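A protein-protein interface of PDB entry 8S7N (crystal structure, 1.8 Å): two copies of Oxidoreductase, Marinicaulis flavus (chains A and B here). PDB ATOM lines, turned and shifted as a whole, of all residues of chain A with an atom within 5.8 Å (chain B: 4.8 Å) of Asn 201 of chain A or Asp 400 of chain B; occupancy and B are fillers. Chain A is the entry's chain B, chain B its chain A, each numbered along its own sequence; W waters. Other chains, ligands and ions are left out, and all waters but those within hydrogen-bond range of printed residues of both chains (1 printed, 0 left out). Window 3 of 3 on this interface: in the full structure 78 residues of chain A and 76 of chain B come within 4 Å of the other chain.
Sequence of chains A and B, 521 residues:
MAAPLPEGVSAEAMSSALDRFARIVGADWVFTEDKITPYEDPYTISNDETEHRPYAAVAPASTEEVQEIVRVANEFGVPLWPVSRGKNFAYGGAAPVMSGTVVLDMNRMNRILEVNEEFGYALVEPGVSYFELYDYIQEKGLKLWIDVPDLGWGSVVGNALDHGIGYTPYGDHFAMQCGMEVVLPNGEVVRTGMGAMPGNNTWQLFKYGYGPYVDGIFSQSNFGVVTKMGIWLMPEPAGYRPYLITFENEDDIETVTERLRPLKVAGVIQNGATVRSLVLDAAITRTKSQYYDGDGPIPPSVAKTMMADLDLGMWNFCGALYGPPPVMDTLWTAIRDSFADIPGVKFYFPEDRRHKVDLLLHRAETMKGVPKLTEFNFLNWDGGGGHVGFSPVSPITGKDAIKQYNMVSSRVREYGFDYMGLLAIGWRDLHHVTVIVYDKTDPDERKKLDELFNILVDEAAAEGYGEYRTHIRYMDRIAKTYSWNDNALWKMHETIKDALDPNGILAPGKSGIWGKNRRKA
Printed residues of chain B that touch a printed residue of chain A: Pro 395, Asp 400, Gly 464 and Tyr 465.
Hydrophobic or aromatic side chains of chain B within 4 Å of the printed part of chain A: Pro 395 and Tyr 465.
Printed residues of chain A that touch a printed residue of chain B: Gly 199, Asn 200, Asn 201, Thr 202 and Leu 205.
Hydrophobic or aromatic side chains of chain A within 4 Å of the printed part of chain B: Leu 205.
Among the printed residues, no Asp or Glu carboxylate lies within 4 Å of a Lys or Arg side-chain nitrogen of the other chain.
Of chain B, only Pro 395, Asp 400 and Tyr 465 come within 4 Å of Asn 201 of chain A.
Of chain A, only Asn 201 (3.1 Å) comes within 4 Å of Asp 400 of chain B.
Printed residues of chain A within 4 Å of Gly 464 of chain B: Gly 199 and Asn 200.
Printed residues of chain B within 4 Å of Leu 205 of chain A: Pro 395 (3.5 Å).
Gly 398 of chain B touches none of the printed residues of chain A.
No position is printed for both chains.
The side-chain amide nitrogen of Asn 201 of chain A lies within hydrogen-bond range of the side-chain carboxylate of Asp 400 of chain B (3.1 Å).
Gly 199 of chain A touches Gly 464 of chain B.
CA of Asn 200 of chain A touches O of Gly 464 of chain B, at 3.4 Å.
Asn 201 of chain A touches Pro 395 of chain B (OD1 to CG, 3.5 Å).
OD1 of Asn 201 of chain A touches CE1 of Tyr 465 of chain B, 3.8 Å away.
CD of Pro 395 of chain B touches CG2 of Thr 202 of chain A, 3.7 Å away.
CB of Pro 395 of chain B touches CD1 of Leu 205 of chain A, 3.5 Å away.
The side-chain carboxylate of Asp 400 of chain B lies within hydrogen-bond range of the side-chain hydroxyl of Tyr 465 of chain B (2.5 Å).
The side-chain amide oxygen (OD1) of Asn 200 of chain A is in hydrogen-bond range of the backbone NH (N) of Thr 202 of chain A (3.1 Å).
OD1 of Asn 200 of chain A lies within hydrogen-bond range of N of Trp 203 of chain A, 3.0 Å away.
Water W1 lies within hydrogen-bond range of O of Gly 464 of chain B (2.4 Å), OD1 of Asn 201 of chain A (2.7 Å) and OG1 of Thr 202 of chain A (2.9 Å).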
ATOM      1  N   GLY A 199       9.759 -19.833  -8.582  1.00  0.00           N
ATOM      2  CA  GLY A 199      11.180 -20.154  -8.348  1.00  0.00           C
ATOM      3  C   GLY A 199      11.564 -21.563  -8.761  1.00  0.00           C
ATOM      4  O   GLY A 199      12.608 -22.034  -8.293  1.00  0.00           O
ATOM      5  N   ASN A 200      10.768 -22.230  -9.611  1.00  0.00           N
ATOM      6  CA  ASN A 200      11.101 -23.593 -10.083  1.00  0.00           C
ATOM      7  C   ASN A 200      12.392 -23.572 -10.900  1.00  0.00           C
ATOM      8  O   ASN A 200      12.727 -22.526 -11.527  1.00  0.00           O
ATOM      9  CB  ASN A 200       9.989 -24.177 -10.962  1.00  0.00           C
ATOM     10  CG  ASN A 200       9.945 -23.560 -12.329  1.00  0.00           C
ATOM     11  OD1 ASN A 200      10.608 -24.050 -13.259  1.00  0.00           O
ATOM     12  ND2 ASN A 200       9.180 -22.473 -12.460  1.00  0.00           N
ATOM     13  N   ASN A 201      12.999 -24.741 -11.042  1.00  0.00           N
ATOM     14  CA  ASN A 201      14.115 -24.965 -11.976  1.00  0.00           C
ATOM     15  C   ASN A 201      13.784 -26.200 -12.815  1.00  0.00           C
ATOM     16  O   ASN A 201      14.723 -26.837 -13.285  1.00  0.00           O
ATOM     17  CB  ASN A 201      15.469 -25.092 -11.250  1.00  0.00           C
ATOM     18  CG  ASN A 201      15.550 -26.140 -10.152  1.00  0.00           C
ATOM     19  OD1 ASN A 201      14.579 -26.846  -9.799  1.00  0.00           O
ATOM     20  ND2 ASN A 201      16.697 -26.145  -9.476  1.00  0.00           N
ATOM     21  N   THR A 202      12.508 -26.442 -13.105  1.00  0.00           N
ATOM     22  CA  THR A 202      12.084 -27.713 -13.726  1.00  0.00           C
ATOM     23  C   THR A 202      11.051 -27.505 -14.838  1.00  0.00           C
ATOM     24  O   THR A 202      10.599 -28.545 -15.365  1.00  0.00           O
ATOM     25  CB  THR A 202      11.554 -28.656 -12.648  1.00  0.00           C
ATOM     26  OG1 THR A 202      10.695 -27.912 -11.784  1.00  0.00           O
ATOM     27  CG2 THR A 202      12.665 -29.298 -11.821  1.00  0.00           C
ATOM     28  N   TRP A 203      10.759 -26.272 -15.259  1.00  0.00           N
ATOM     29  CA  TRP A 203       9.689 -26.010 -16.279  1.00  0.00           C
ATOM     30  C   TRP A 203       9.919 -26.821 -17.566  1.00  0.00           C
ATOM     31  O   TRP A 203       8.970 -27.374 -18.151  1.00  0.00           O
ATOM     32  CB  TRP A 203       9.658 -24.516 -16.620  1.00  0.00           C
ATOM     33  CG  TRP A 203       8.417 -24.044 -17.294  1.00  0.00           C
ATOM     34  CD1 TRP A 203       7.217 -24.698 -17.380  1.00  0.00           C
ATOM     35  CD2 TRP A 203       8.232 -22.761 -17.921  1.00  0.00           C
ATOM     36  NE1 TRP A 203       6.301 -23.896 -18.002  1.00  0.00           N
ATOM     37  CE2 TRP A 203       6.874 -22.682 -18.297  1.00  0.00           C
ATOM     38  CE3 TRP A 203       9.061 -21.654 -18.130  1.00  0.00           C
ATOM     39  CZ2 TRP A 203       6.351 -21.568 -18.966  1.00  0.00           C
ATOM     40  CZ3 TRP A 203       8.511 -20.515 -18.677  1.00  0.00           C
ATOM     41  CH2 TRP A 203       7.191 -20.485 -19.121  1.00  0.00           C
ATOM     42  N   LEU A 205      11.978 -29.493 -17.706  1.00  0.00           N
ATOM     43  CA  LEU A 205      12.505 -30.817 -17.293  1.00  0.00           C
ATOM     44  C   LEU A 205      11.388 -31.861 -17.049  1.00  0.00           C
ATOM     45  O   LEU A 205      11.650 -33.068 -17.240  1.00  0.00           O
ATOM     46  CB  LEU A 205      13.320 -30.604 -16.027  1.00  0.00           C
ATOM     47  CG  LEU A 205      14.561 -29.706 -16.183  1.00  0.00           C
ATOM     48  CD1 LEU A 205      15.479 -29.862 -14.986  1.00  0.00           C
ATOM     49  CD2 LEU A 205      15.313 -30.032 -17.433  1.00  0.00           C
ATOM     50  N   SER B 394      12.872 -33.062  -9.021  1.00  0.00           N
ATOM     51  CA  SER B 394      14.226 -32.452  -9.029  1.00  0.00           C
ATOM     52  C   SER B 394      14.762 -32.455 -10.451  1.00  0.00           C
ATOM     53  O   SER B 394      14.521 -33.408 -11.205  1.00  0.00           O
ATOM     54  CB  SER B 394      15.137 -33.244  -8.064  1.00  0.00           C
ATOM     55  OG  SER B 394      16.483 -32.845  -8.185  1.00  0.00           O
ATOM     56  N   PRO B 395      15.565 -31.453 -10.847  1.00  0.00           N
ATOM     57  CA  PRO B 395      16.467 -31.625 -11.981  1.00  0.00           C
ATOM     58  C   PRO B 395      17.390 -32.835 -11.746  1.00  0.00           C
ATOM     59  O   PRO B 395      17.699 -33.156 -10.573  1.00  0.00           O
ATOM     60  CB  PRO B 395      17.337 -30.365 -12.009  1.00  0.00           C
ATOM     61  CG  PRO B 395      16.545 -29.381 -11.160  1.00  0.00           C
ATOM     62  CD  PRO B 395      15.837 -30.214 -10.127  1.00  0.00           C
ATOM     63  N   THR B 397      20.467 -33.038 -11.394  1.00  0.00           N
ATOM     64  CA  THR B 397      21.642 -32.252 -10.986  1.00  0.00           C
ATOM     65  C   THR B 397      22.083 -32.713  -9.601  1.00  0.00           C
ATOM     66  O   THR B 397      21.224 -32.759  -8.737  1.00  0.00           O
ATOM     67  CB  THR B 397      21.240 -30.769 -10.971  1.00  0.00           C
ATOM     68  OG1 THR B 397      20.934 -30.324 -12.297  1.00  0.00           O
ATOM     69  CG2 THR B 397      22.325 -29.904 -10.396  1.00  0.00           C
ATOM     70  N   GLY B 398      23.371 -32.944  -9.405  1.00  0.00           N
ATOM     71  CA  GLY B 398      23.927 -33.317  -8.100  1.00  0.00           C
ATOM     72  C   GLY B 398      23.509 -32.350  -7.016  1.00  0.00           C
ATOM     73  O   GLY B 398      23.151 -32.784  -5.946  1.00  0.00           O
ATOM     74  N   LYS B 399      23.559 -31.049  -7.295  1.00  0.00           N
ATOM     75  CA  LYS B 399      23.326 -30.020  -6.270  1.00  0.00           C
ATOM     76  C   LYS B 399      21.906 -30.165  -5.750  1.00  0.00           C
ATOM     77  O   LYS B 399      21.716 -30.037  -4.511  1.00  0.00           O
ATOM     78  CB  LYS B 399      23.597 -28.628  -6.852  1.00  0.00           C
ATOM     79  CG  LYS B 399      23.200 -27.456  -5.966  1.00  0.00           C
ATOM     80  CD  LYS B 399      23.363 -26.161  -6.765  1.00  0.00           C
ATOM     81  CE  LYS B 399      22.799 -24.971  -6.049  1.00  0.00           C
ATOM     82  NZ  LYS B 399      23.763 -24.510  -5.026  1.00  0.00           N
ATOM     83  N   ASP B 400      20.937 -30.346  -6.653  1.00  0.00           N
ATOM     84  CA  ASP B 400      19.515 -30.477  -6.267  1.00  0.00           C
ATOM     85  C   ASP B 400      19.286 -31.798  -5.504  1.00  0.00           C
ATOM     86  O   ASP B 400      18.497 -31.808  -4.556  1.00  0.00           O
ATOM     87  CB  ASP B 400      18.579 -30.315  -7.468  1.00  0.00           C
ATOM     88  CG  ASP B 400      18.689 -28.923  -8.056  1.00  0.00           C
ATOM     89  OD1 ASP B 400      18.089 -27.999  -7.474  1.00  0.00           O
ATOM     90  OD2 ASP B 400      19.403 -28.789  -9.040  1.00  0.00           O
ATOM     91  N   ALA B 401      19.840 -32.881  -5.989  1.00  0.00           N
ATOM     92  CA  ALA B 401      19.584 -34.225  -5.423  1.00  0.00           C
ATOM     93  C   ALA B 401      20.144 -34.238  -4.003  1.00  0.00           C
ATOM     94  O   ALA B 401      19.433 -34.632  -3.097  1.00  0.00           O
ATOM     95  CB  ALA B 401      20.231 -35.285  -6.274  1.00  0.00           C
ATOM     96  N   ILE B 402      21.352 -33.734  -3.800  1.00  0.00           N
ATOM     97  CA  ILE B 402      21.915 -33.757  -2.422  1.00  0.00           C
ATOM     98  C   ILE B 402      21.204 -32.718  -1.534  1.00  0.00           C
ATOM     99  O   ILE B 402      21.022 -33.012  -0.334  1.00  0.00           O
ATOM    100  CB  ILE B 402      23.442 -33.675  -2.407  1.00  0.00           C
ATOM    101  CG1 ILE B 402      23.983 -34.188  -1.072  1.00  0.00           C
ATOM    102  CG2 ILE B 402      23.910 -32.257  -2.712  1.00  0.00           C
ATOM    103  CD1 ILE B 402      25.497 -34.410  -1.060  1.00  0.00           C
ATOM    104  N   LYS B 403      20.766 -31.574  -2.068  1.00  0.00           N
ATOM    105  CA  LYS B 403      19.974 -30.592  -1.290  1.00  0.00           C
ATOM    106  C   LYS B 403      18.692 -31.285  -0.804  1.00  0.00           C
ATOM    107  O   LYS B 403      18.363 -31.152   0.383  1.00  0.00           O
ATOM    108  CB  LYS B 403      19.681 -29.361  -2.150  1.00  0.00           C
ATOM    109  CG  LYS B 403      18.784 -28.282  -1.554  1.00  0.00           C
ATOM    110  CD  LYS B 403      19.217 -27.823  -0.185  1.00  0.00           C
ATOM    111  CE  LYS B 403      18.575 -26.525   0.283  1.00  0.00           C
ATOM    112  NZ  LYS B 403      19.238 -25.953   1.483  1.00  0.00           N
ATOM    113  N   GLN B 404      17.974 -31.977  -1.702  1.00  0.00           N
ATOM    114  CA  GLN B 404      16.675 -32.607  -1.335  1.00  0.00           C
ATOM    115  C   GLN B 404      16.941 -33.720  -0.296  1.00  0.00           C
ATOM    116  O   GLN B 404      16.154 -33.856   0.643  1.00  0.00           O
ATOM    117  CB  GLN B 404      15.929 -33.141  -2.556  1.00  0.00           C
ATOM    118  CG  GLN B 404      15.340 -32.033  -3.417  1.00  0.00           C
ATOM    119  CD  GLN B 404      14.309 -32.498  -4.413  1.00  0.00           C
ATOM    120  OE1 GLN B 404      13.877 -33.640  -4.388  1.00  0.00           O
ATOM    121  NE2 GLN B 404      13.838 -31.563  -5.244  1.00  0.00           N
ATOM    122  N   GLY B 464      11.666 -23.899  -4.269  1.00  0.00           N
ATOM    123  CA  GLY B 464      11.261 -23.988  -5.688  1.00  0.00           C
ATOM    124  C   GLY B 464      11.040 -25.422  -6.141  1.00  0.00           C
ATOM    125  O   GLY B 464      11.150 -25.705  -7.382  1.00  0.00           O
ATOM    126  N   TYR B 465      10.721 -26.321  -5.196  1.00  0.00           N
ATOM    127  CA  TYR B 465      10.484 -27.758  -5.530  1.00  0.00           C
ATOM    128  C   TYR B 465       9.008 -28.095  -5.266  1.00  0.00           C
ATOM    129  O   TYR B 465       8.464 -27.790  -4.197  1.00  0.00           O
ATOM    130  CB  TYR B 465      11.427 -28.713  -4.782  1.00  0.00           C
ATOM    131  CG  TYR B 465      12.921 -28.510  -4.928  1.00  0.00           C
ATOM    132  CD1 TYR B 465      13.540 -28.427  -6.162  1.00  0.00           C
ATOM    133  CD2 TYR B 465      13.725 -28.431  -3.786  1.00  0.00           C
ATOM    134  CE1 TYR B 465      14.911 -28.313  -6.276  1.00  0.00           C
ATOM    135  CE2 TYR B 465      15.095 -28.265  -3.884  1.00  0.00           C
ATOM    136  CZ  TYR B 465      15.686 -28.213  -5.125  1.00  0.00           C
ATOM    137  OH  TYR B 465      17.025 -28.101  -5.205  1.00  0.00           O
HETATM  138  O   HOH W   1      11.934 -27.069  -9.246  1.00  0.00           O
